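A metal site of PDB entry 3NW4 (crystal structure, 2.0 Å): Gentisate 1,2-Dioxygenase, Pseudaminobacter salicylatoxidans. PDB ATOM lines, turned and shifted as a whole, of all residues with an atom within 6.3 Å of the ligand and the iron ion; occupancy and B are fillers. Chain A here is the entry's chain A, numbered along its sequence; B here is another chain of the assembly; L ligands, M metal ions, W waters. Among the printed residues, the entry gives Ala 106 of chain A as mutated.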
ATOM      1  N   GLU A  82     -32.988 -21.663 -18.722  1.00  0.00           N
ATOM      2  CA  GLU A  82     -32.572 -21.483 -20.156  1.00  0.00           C
ATOM      3  C   GLU A  82     -31.501 -22.422 -20.727  1.00  0.00           C
ATOM      4  O   GLU A  82     -31.683 -22.989 -21.828  1.00  0.00           O
ATOM      5  CB  GLU A  82     -32.236 -20.014 -20.483  1.00  0.00           C
ATOM      6  CG  GLU A  82     -33.418 -19.056 -20.267  1.00  0.00           C
ATOM      7  CD  GLU A  82     -34.596 -19.307 -21.252  1.00  0.00           C
ATOM      8  OE1 GLU A  82     -34.420 -19.047 -22.473  1.00  0.00           O
ATOM      9  OE2 GLU A  82     -35.677 -19.765 -20.779  1.00  0.00           O
ATOM     10  N   ARG A  83     -30.375 -22.582 -20.004  1.00  0.00           N
ATOM     11  CA  ARG A  83     -29.200 -23.321 -20.487  1.00  0.00           C
ATOM     12  C   ARG A  83     -28.567 -24.093 -19.344  1.00  0.00           C
ATOM     13  O   ARG A  83     -28.498 -23.600 -18.234  1.00  0.00           O
ATOM     14  CB  ARG A  83     -28.133 -22.322 -21.029  1.00  0.00           C
ATOM     15  CG  ARG A  83     -28.648 -21.279 -22.046  1.00  0.00           C
ATOM     16  CD  ARG A  83     -28.973 -21.928 -23.371  1.00  0.00           C
ATOM     17  NE  ARG A  83     -29.378 -21.009 -24.435  1.00  0.00           N
ATOM     18  CZ  ARG A  83     -30.637 -20.866 -24.854  1.00  0.00           C
ATOM     19  NH1 ARG A  83     -31.606 -21.562 -24.253  1.00  0.00           N
ATOM     20  NH2 ARG A  83     -30.924 -20.067 -25.887  1.00  0.00           N
ATOM     21  N   ALA A  85     -25.533 -24.406 -18.322  1.00  0.00           N
ATOM     22  CA  ALA A  85     -24.207 -23.816 -18.450  1.00  0.00           C
ATOM     23  C   ALA A  85     -23.626 -23.617 -17.058  1.00  0.00           C
ATOM     24  O   ALA A  85     -24.303 -23.114 -16.156  1.00  0.00           O
ATOM     25  CB  ALA A  85     -24.279 -22.451 -19.235  1.00  0.00           C
ATOM     26  N   LEU A  86     -22.384 -24.007 -16.880  1.00  0.00           N
ATOM     27  CA  LEU A  86     -21.739 -23.949 -15.559  1.00  0.00           C
ATOM     28  C   LEU A  86     -20.707 -22.838 -15.659  1.00  0.00           C
ATOM     29  O   LEU A  86     -19.659 -22.995 -16.322  1.00  0.00           O
ATOM     30  CB  LEU A  86     -21.050 -25.292 -15.241  1.00  0.00           C
ATOM     31  CG  LEU A  86     -21.807 -26.595 -14.895  1.00  0.00           C
ATOM     32  CD1 LEU A  86     -22.758 -26.998 -16.013  1.00  0.00           C
ATOM     33  CD2 LEU A  86     -20.831 -27.763 -14.661  1.00  0.00           C
ATOM     34  N   TRP A 104     -17.937 -13.455 -18.728  1.00  0.00           N
ATOM     35  CA  TRP A 104     -18.453 -14.766 -18.312  1.00  0.00           C
ATOM     36  C   TRP A 104     -17.890 -15.865 -19.228  1.00  0.00           C
ATOM     37  O   TRP A 104     -17.720 -15.650 -20.412  1.00  0.00           O
ATOM     38  CB  TRP A 104     -19.983 -14.751 -18.381  1.00  0.00           C
ATOM     39  CG  TRP A 104     -20.673 -16.109 -18.482  1.00  0.00           C
ATOM     40  CD1 TRP A 104     -20.770 -16.900 -19.594  1.00  0.00           C
ATOM     41  CD2 TRP A 104     -21.410 -16.762 -17.462  1.00  0.00           C
ATOM     42  NE1 TRP A 104     -21.507 -18.031 -19.313  1.00  0.00           N
ATOM     43  CE2 TRP A 104     -21.914 -17.976 -18.008  1.00  0.00           C
ATOM     44  CE3 TRP A 104     -21.732 -16.434 -16.133  1.00  0.00           C
ATOM     45  CZ2 TRP A 104     -22.711 -18.863 -17.275  1.00  0.00           C
ATOM     46  CZ3 TRP A 104     -22.521 -17.324 -15.389  1.00  0.00           C
ATOM     47  CH2 TRP A 104     -23.008 -18.525 -15.970  1.00  0.00           C
ATOM     48  N   ALA A 105     -17.544 -17.019 -18.633  1.00  0.00           N
ATOM     49  CA  ALA A 105     -17.150 -18.217 -19.388  1.00  0.00           C
ATOM     50  C   ALA A 105     -17.838 -19.406 -18.743  1.00  0.00           C
ATOM     51  O   ALA A 105     -17.974 -19.470 -17.531  1.00  0.00           O
ATOM     52  CB  ALA A 105     -15.655 -18.419 -19.337  1.00  0.00           C
ATOM     53  N   ALA A 106     -18.278 -20.366 -19.553  1.00  0.00           N
ATOM     54  CA  ALA A 106     -19.001 -21.472 -19.002  1.00  0.00           C
ATOM     55  C   ALA A 106     -18.739 -22.680 -19.815  1.00  0.00           C
ATOM     56  O   ALA A 106     -18.524 -22.572 -21.018  1.00  0.00           O
ATOM     57  CB  ALA A 106     -20.512 -21.186 -19.026  1.00  0.00           C
ATOM     58  N   GLN A 108     -20.972 -25.583 -21.248  1.00  0.00           N
ATOM     59  CA  GLN A 108     -22.378 -25.878 -21.438  1.00  0.00           C
ATOM     60  C   GLN A 108     -22.509 -27.310 -21.955  1.00  0.00           C
ATOM     61  O   GLN A 108     -21.689 -27.778 -22.746  1.00  0.00           O
ATOM     62  CB  GLN A 108     -23.071 -24.879 -22.361  1.00  0.00           C
ATOM     63  CG  GLN A 108     -24.568 -25.236 -22.545  1.00  0.00           C
ATOM     64  CD  GLN A 108     -25.365 -24.202 -23.280  1.00  0.00           C
ATOM     65  OE1 GLN A 108     -24.914 -23.062 -23.489  1.00  0.00           O
ATOM     66  NE2 GLN A 108     -26.555 -24.556 -23.659  1.00  0.00           N
ATOM     67  N   HIS A 119     -34.016 -17.464 -27.236  1.00  0.00           N
ATOM     68  CA  HIS A 119     -34.158 -16.178 -26.537  1.00  0.00           C
ATOM     69  C   HIS A 119     -33.206 -15.153 -27.174  1.00  0.00           C
ATOM     70  O   HIS A 119     -32.432 -15.507 -28.061  1.00  0.00           O
ATOM     71  CB  HIS A 119     -33.927 -16.339 -25.030  1.00  0.00           C
ATOM     72  CG  HIS A 119     -32.526 -16.709 -24.657  1.00  0.00           C
ATOM     73  ND1 HIS A 119     -32.250 -17.576 -23.618  1.00  0.00           N
ATOM     74  CD2 HIS A 119     -31.326 -16.335 -25.172  1.00  0.00           C
ATOM     75  CE1 HIS A 119     -30.936 -17.742 -23.520  1.00  0.00           C
ATOM     76  NE2 HIS A 119     -30.355 -17.009 -24.463  1.00  0.00           N
ATOM     77  N   ARG A 120     -33.279 -13.881 -26.759  1.00  0.00           N
ATOM     78  CA  ARG A 120     -32.245 -12.909 -27.165  1.00  0.00           C
ATOM     79  C   ARG A 120     -31.974 -11.971 -26.015  1.00  0.00           C
ATOM     80  O   ARG A 120     -32.808 -11.805 -25.119  1.00  0.00           O
ATOM     81  CB  ARG A 120     -32.625 -12.124 -28.422  1.00  0.00           C
ATOM     82  CG  ARG A 120     -33.851 -11.198 -28.247  1.00  0.00           C
ATOM     83  CD  ARG A 120     -34.168 -10.499 -29.578  1.00  0.00           C
ATOM     84  NE  ARG A 120     -35.418  -9.736 -29.550  1.00  0.00           N
ATOM     85  CZ  ARG A 120     -35.899  -9.018 -30.569  1.00  0.00           C
ATOM     86  NH1 ARG A 120     -37.071  -8.394 -30.459  1.00  0.00           N
ATOM     87  NH2 ARG A 120     -35.247  -8.952 -31.714  1.00  0.00           N
ATOM     88  N   HIS A 121     -30.808 -11.331 -26.044  1.00  0.00           N
ATOM     89  CA  HIS A 121     -30.401 -10.419 -24.976  1.00  0.00           C
ATOM     90  C   HIS A 121     -29.360  -9.446 -25.478  1.00  0.00           C
ATOM     91  O   HIS A 121     -28.680  -9.726 -26.472  1.00  0.00           O
ATOM     92  CB  HIS A 121     -29.888 -11.227 -23.780  1.00  0.00           C
ATOM     93  CG  HIS A 121     -29.120 -12.451 -24.169  1.00  0.00           C
ATOM     94  ND1 HIS A 121     -27.873 -12.397 -24.757  1.00  0.00           N
ATOM     95  CD2 HIS A 121     -29.415 -13.768 -24.030  1.00  0.00           C
ATOM     96  CE1 HIS A 121     -27.437 -13.636 -24.982  1.00  0.00           C
ATOM     97  NE2 HIS A 121     -28.355 -14.480 -24.554  1.00  0.00           N
ATOM     98  N   ALA A 125     -22.308 -12.743 -27.253  1.00  0.00           N
ATOM     99  CA  ALA A 125     -21.963 -14.107 -26.882  1.00  0.00           C
ATOM    100  C   ALA A 125     -21.267 -14.841 -28.003  1.00  0.00           C
ATOM    101  O   ALA A 125     -21.507 -14.555 -29.166  1.00  0.00           O
ATOM    102  CB  ALA A 125     -23.272 -14.927 -26.479  1.00  0.00           C
ATOM    103  N   ARG A 127     -19.672 -19.170 -28.900  1.00  0.00           N
ATOM    104  CA  ARG A 127     -19.470 -20.576 -28.526  1.00  0.00           C
ATOM    105  C   ARG A 127     -18.131 -21.089 -29.083  1.00  0.00           C
ATOM    106  O   ARG A 127     -17.802 -20.859 -30.246  1.00  0.00           O
ATOM    107  CB  ARG A 127     -20.589 -21.471 -29.105  1.00  0.00           C
ATOM    108  CG  ARG A 127     -21.975 -20.815 -29.224  1.00  0.00           C
ATOM    109  CD  ARG A 127     -22.527 -20.439 -27.863  1.00  0.00           C
ATOM    110  NE  ARG A 127     -23.725 -19.598 -27.960  1.00  0.00           N
ATOM    111  CZ  ARG A 127     -24.155 -18.821 -26.973  1.00  0.00           C
ATOM    112  NH1 ARG A 127     -23.446 -18.766 -25.847  1.00  0.00           N
ATOM    113  NH2 ARG A 127     -25.240 -18.076 -27.139  1.00  0.00           N
ATOM    114  N   THR A 154     -22.926 -15.292 -31.565  1.00  0.00           N
ATOM    115  CA  THR A 154     -24.303 -14.860 -31.429  1.00  0.00           C
ATOM    116  C   THR A 154     -24.305 -13.441 -30.842  1.00  0.00           C
ATOM    117  O   THR A 154     -24.316 -13.250 -29.606  1.00  0.00           O
ATOM    118  CB  THR A 154     -25.268 -15.914 -30.771  1.00  0.00           C
ATOM    119  OG1 THR A 154     -26.338 -15.264 -30.066  1.00  0.00           O
ATOM    120  CG2 THR A 154     -24.523 -16.833 -29.855  1.00  0.00           C
ATOM    121  N   HIS A 160     -31.491 -16.890 -30.518  1.00  0.00           N
ATOM    122  CA  HIS A 160     -30.714 -18.110 -30.604  1.00  0.00           C
ATOM    123  C   HIS A 160     -31.314 -19.178 -29.708  1.00  0.00           C
ATOM    124  O   HIS A 160     -31.798 -18.887 -28.612  1.00  0.00           O
ATOM    125  CB  HIS A 160     -29.224 -17.885 -30.253  1.00  0.00           C
ATOM    126  CG  HIS A 160     -28.982 -17.247 -28.913  1.00  0.00           C
ATOM    127  ND1 HIS A 160     -29.269 -15.919 -28.674  1.00  0.00           N
ATOM    128  CD2 HIS A 160     -28.454 -17.732 -27.761  1.00  0.00           C
ATOM    129  CE1 HIS A 160     -28.916 -15.610 -27.432  1.00  0.00           C
ATOM    130  NE2 HIS A 160     -28.416 -16.683 -26.858  1.00  0.00           N
ATOM    131  N   HIS A 162     -30.666 -23.887 -29.374  1.00  0.00           N
ATOM    132  CA  HIS A 162     -29.806 -24.994 -29.836  1.00  0.00           C
ATOM    133  C   HIS A 162     -30.499 -26.320 -29.626  1.00  0.00           C
ATOM    134  O   HIS A 162     -31.325 -26.448 -28.704  1.00  0.00           O
ATOM    135  CB  HIS A 162     -28.472 -25.117 -29.086  1.00  0.00           C
ATOM    136  CG  HIS A 162     -28.075 -23.930 -28.267  1.00  0.00           C
ATOM    137  ND1 HIS A 162     -27.995 -23.981 -26.897  1.00  0.00           N
ATOM    138  CD2 HIS A 162     -27.640 -22.697 -28.628  1.00  0.00           C
ATOM    139  CE1 HIS A 162     -27.578 -22.817 -26.437  1.00  0.00           C
ATOM    140  NE2 HIS A 162     -27.359 -22.018 -27.460  1.00  0.00           N
ATOM    141  N   TRP A 172     -19.429 -27.669 -24.873  1.00  0.00           N
ATOM    142  CA  TRP A 172     -18.629 -26.578 -25.459  1.00  0.00           C
ATOM    143  C   TRP A 172     -18.442 -25.481 -24.417  1.00  0.00           C
ATOM    144  O   TRP A 172     -18.920 -25.617 -23.278  1.00  0.00           O
ATOM    145  CB  TRP A 172     -19.314 -26.008 -26.704  1.00  0.00           C
ATOM    146  CG  TRP A 172     -20.670 -25.346 -26.462  1.00  0.00           C
ATOM    147  CD1 TRP A 172     -20.917 -24.037 -26.158  1.00  0.00           C
ATOM    148  CD2 TRP A 172     -21.948 -25.997 -26.487  1.00  0.00           C
ATOM    149  NE1 TRP A 172     -22.271 -23.814 -26.027  1.00  0.00           N
ATOM    150  CE2 TRP A 172     -22.933 -25.015 -26.241  1.00  0.00           C
ATOM    151  CE3 TRP A 172     -22.363 -27.324 -26.715  1.00  0.00           C
ATOM    152  CZ2 TRP A 172     -24.318 -25.316 -26.193  1.00  0.00           C
ATOM    153  CZ3 TRP A 172     -23.749 -27.625 -26.667  1.00  0.00           C
ATOM    154  CH2 TRP A 172     -24.702 -26.617 -26.428  1.00  0.00           C
ATOM    155  N   ASP A 174     -18.998 -21.332 -23.591  1.00  0.00           N
ATOM    156  CA  ASP A 174     -19.647 -20.106 -23.900  1.00  0.00           C
ATOM    157  C   ASP A 174     -18.756 -18.992 -23.357  1.00  0.00           C
ATOM    158  O   ASP A 174     -18.209 -19.144 -22.277  1.00  0.00           O
ATOM    159  CB  ASP A 174     -20.944 -19.965 -23.145  1.00  0.00           C
ATOM    160  CG  ASP A 174     -21.942 -20.997 -23.484  1.00  0.00           C
ATOM    161  OD1 ASP A 174     -22.159 -21.245 -24.692  1.00  0.00           O
ATOM    162  OD2 ASP A 174     -22.567 -21.525 -22.530  1.00  0.00           O
ATOM    163  N   GLY A 175     -18.650 -17.884 -24.097  1.00  0.00           N
ATOM    164  CA  GLY A 175     -18.150 -16.614 -23.531  1.00  0.00           C
ATOM    165  C   GLY A 175     -19.178 -15.529 -23.750  1.00  0.00           C
ATOM    166  O   GLY A 175     -19.763 -15.459 -24.844  1.00  0.00           O
ATOM    167  N   LEU A 176     -19.401 -14.683 -22.737  1.00  0.00           N
ATOM    168  CA  LEU A 176     -20.322 -13.525 -22.869  1.00  0.00           C
ATOM    169  C   LEU A 176     -19.770 -12.310 -22.132  1.00  0.00           C
ATOM    170  O   LEU A 176     -18.868 -12.430 -21.292  1.00  0.00           O
ATOM    171  CB  LEU A 176     -21.741 -13.817 -22.329  1.00  0.00           C
ATOM    172  CG  LEU A 176     -22.696 -14.761 -23.102  1.00  0.00           C
ATOM    173  CD1 LEU A 176     -22.500 -16.247 -22.682  1.00  0.00           C
ATOM    174  CD2 LEU A 176     -24.148 -14.366 -22.938  1.00  0.00           C
ATOM    175  N   ILE A 178     -21.553 -10.794 -19.983  1.00  0.00           N
ATOM    176  CA  ILE A 178     -22.464 -10.749 -18.810  1.00  0.00           C
ATOM    177  C   ILE A 178     -22.008  -9.856 -17.613  1.00  0.00           C
ATOM    178  O   ILE A 178     -22.784  -9.017 -17.156  1.00  0.00           O
ATOM    179  CB  ILE A 178     -22.874 -12.204 -18.352  1.00  0.00           C
ATOM    180  CG1 ILE A 178     -23.989 -12.769 -19.276  1.00  0.00           C
ATOM    181  CG2 ILE A 178     -23.321 -12.246 -16.863  1.00  0.00           C
ATOM    182  CD1 ILE A 178     -24.186 -14.314 -19.103  1.00  0.00           C
ATOM    183  N   PHE A 189     -33.412  -8.451 -22.134  1.00  0.00           N
ATOM    184  CA  PHE A 189     -33.580  -9.883 -22.378  1.00  0.00           C
ATOM    185  C   PHE A 189     -35.027 -10.143 -22.863  1.00  0.00           C
ATOM    186  O   PHE A 189     -35.972  -9.525 -22.352  1.00  0.00           O
ATOM    187  CB  PHE A 189     -33.314 -10.682 -21.102  1.00  0.00           C
ATOM    188  CG  PHE A 189     -33.474 -12.172 -21.269  1.00  0.00           C
ATOM    189  CD1 PHE A 189     -34.761 -12.756 -21.304  1.00  0.00           C
ATOM    190  CD2 PHE A 189     -32.349 -13.005 -21.396  1.00  0.00           C
ATOM    191  CE1 PHE A 189     -34.936 -14.157 -21.453  1.00  0.00           C
ATOM    192  CE2 PHE A 189     -32.501 -14.412 -21.554  1.00  0.00           C
ATOM    193  CZ  PHE A 189     -33.819 -14.977 -21.588  1.00  0.00           C
ATOM    194  N   LEU B  38     -25.666 -21.330 -14.336  1.00  0.00           N
ATOM    195  CA  LEU B  38     -26.527 -20.261 -14.876  1.00  0.00           C
ATOM    196  C   LEU B  38     -27.982 -20.429 -14.428  1.00  0.00           C
ATOM    197  O   LEU B  38     -28.688 -19.438 -14.153  1.00  0.00           O
ATOM    198  CB  LEU B  38     -26.488 -20.220 -16.412  1.00  0.00           C
ATOM    199  CG  LEU B  38     -27.333 -19.140 -17.107  1.00  0.00           C
ATOM    200  CD1 LEU B  38     -26.695 -17.734 -16.943  1.00  0.00           C
ATOM    201  CD2 LEU B  38     -27.489 -19.507 -18.605  1.00  0.00           C
ATOM    202  N   LEU B  42     -30.070 -17.056 -13.619  1.00  0.00           N
ATOM    203  CA  LEU B  42     -30.375 -16.462 -14.952  1.00  0.00           C
ATOM    204  C   LEU B  42     -30.989 -15.066 -14.884  1.00  0.00           C
ATOM    205  O   LEU B  42     -30.471 -14.154 -15.527  1.00  0.00           O
ATOM    206  CB  LEU B  42     -31.225 -17.372 -15.868  1.00  0.00           C
ATOM    207  CG  LEU B  42     -31.226 -16.804 -17.310  1.00  0.00           C
ATOM    208  CD1 LEU B  42     -30.507 -17.711 -18.262  1.00  0.00           C
ATOM    209  CD2 LEU B  42     -32.577 -16.466 -17.857  1.00  0.00           C
ATOM    210  N   MET B  46     -29.303 -11.562 -16.154  1.00  0.00           N
ATOM    211  CA  MET B  46     -29.803 -11.115 -17.466  1.00  0.00           C
ATOM    212  C   MET B  46     -31.237 -10.604 -17.418  1.00  0.00           C
ATOM    213  O   MET B  46     -32.169 -11.257 -17.924  1.00  0.00           O
ATOM    214  CB  MET B  46     -29.653 -12.240 -18.514  1.00  0.00           C
ATOM    215  CG  MET B  46     -28.231 -12.862 -18.549  1.00  0.00           C
ATOM    216  SD  MET B  46     -28.049 -14.112 -19.841  1.00  0.00           S
ATOM    217  CE  MET B  46     -27.451 -13.087 -21.140  1.00  0.00           C
HETATM  218  O1  LIG L   1     -27.583 -18.635 -24.917  1.00  0.00           O
HETATM  219  O2  LIG L   1     -26.372 -20.547 -24.659  1.00  0.00           O
HETATM  220  O3  LIG L   1     -23.305 -19.707 -20.808  1.00  0.00           O
HETATM  221  O4  LIG L   1     -27.658 -16.943 -22.913  1.00  0.00           O
HETATM  222  C1  LIG L   1     -24.877 -17.912 -20.674  1.00  0.00           C
HETATM  223  C2  LIG L   1     -25.958 -17.197 -21.214  1.00  0.00           C
HETATM  224  C3  LIG L   1     -24.954 -19.513 -22.509  1.00  0.00           C
HETATM  225  C4  LIG L   1     -26.709 -19.360 -24.296  1.00  0.00           C
HETATM  226  C5  LIG L   1     -24.368 -19.049 -21.334  1.00  0.00           C
HETATM  227  C6  LIG L   1     -26.576 -17.632 -22.385  1.00  0.00           C
HETATM  228  C7  LIG L   1     -26.053 -18.839 -23.057  1.00  0.00           C
HETATM  229 FE    FE M   1     -28.160 -16.702 -24.738  1.00  0.00          FE
HETATM  230  O   HOH W   1     -25.784 -16.562 -25.170  1.00  0.00           O
HETATM  231  O   HOH W   2     -29.555 -16.513 -20.986  1.00  0.00           O
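The iron ion is bound by an oxygen (O4) of the ligand (1.9 Å), an oxygen (O1) of the ligand (2.0 Å), a ring nitrogen (NE2) of His 160 (2.1 Å), a ring nitrogen (NE2) of His 119 (2.2 Å), a ring nitrogen (NE2) of His 121 (2.2 Å) and water W1 (2.4 Å).
An oxygen (O3) of the ligand is in hydrogen-bond range of the side-chain carboxylate of Asp 174 (2.6 Å).
An oxygen (O2) of the ligand sits close to a ring nitrogen (NE2) of His 162.
An oxygen (O2) of the ligand lies close to the side-chain amide oxygen (OE1) of Gln 108 (3.1 Å).
The guanidinium group (NE) of Arg 83 is in salt-bridge range of an oxygen (O2) of the ligand (3.0 Å).
The indole nitrogen of Trp 104 lies within hydrogen-bond range of an oxygen (O3) of the ligand (2.9 Å).
An oxygen (O2) of the ligand is in salt-bridge range of the guanidinium group (NH1) of Arg 127, at 3.6 Å.
The side-chain carboxylate (OD2) of Asp 174 sits close to the side-chain amide oxygen (OE1) of Gln 108, 3.0 Å away.
The guanidinium group (NH2) of Arg 83 sits close to a ring nitrogen (NE2) of His 119, at 3.4 Å.
The side-chain carboxylate (OD1) of Asp 174 is in salt-bridge range of the guanidinium group (NH1) of Arg 127 (3.0 Å).
O of Ala 85 sits at hydrogen-bond distance from N of Leu 38 of chain B, at 2.9 Å.
A ring nitrogen (NE2) of His 160 lies close to the guanidinium group (NH2) of Arg 127, 3.5 Å away.
OG1 of Thr 154 lies within hydrogen-bond range of ND1 of His 160, at 3.3 Å.
The backbone NH (N) of Asp 174 lies within hydrogen-bond range of the backbone carbonyl oxygen (O) of Ala 106, at 2.9 Å.
N of Gln 108 lies within hydrogen-bond range of O of Trp 172, 2.9 Å away.
Within 4 Å of the iron ion: His 119, His 121 and His 160.
Merely in contact with the ligand: Ala 85 (3.3 Å), Ala 106 (3.6 Å), Leu 176 (3.5 Å), Ile 178 (3.99 Å), Leu 38 of chain B (3.7 Å) and Met 46 of chain B (3.97 Å).
Hydrophobic or aromatic side chains within 4 Å of the ligand: Ala 85, Trp 104, Ala 106, His 119, His 121, His 160, His 162, Leu 176, Ile 178, Leu 38 of chain B and Met 46 of chain B.
Within 4 Å of the ligand: Arg 83, Ala 85, Trp 104, Ala 106, Gln 108, His 119, His 121, Arg 127, His 160, His 162, Asp 174, Leu 176, Ile 178, Leu 38 of chain B and Met 46 of chain B.
The nearest printed residue that does not touch the ligand is Trp 172 (5.4 Å).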
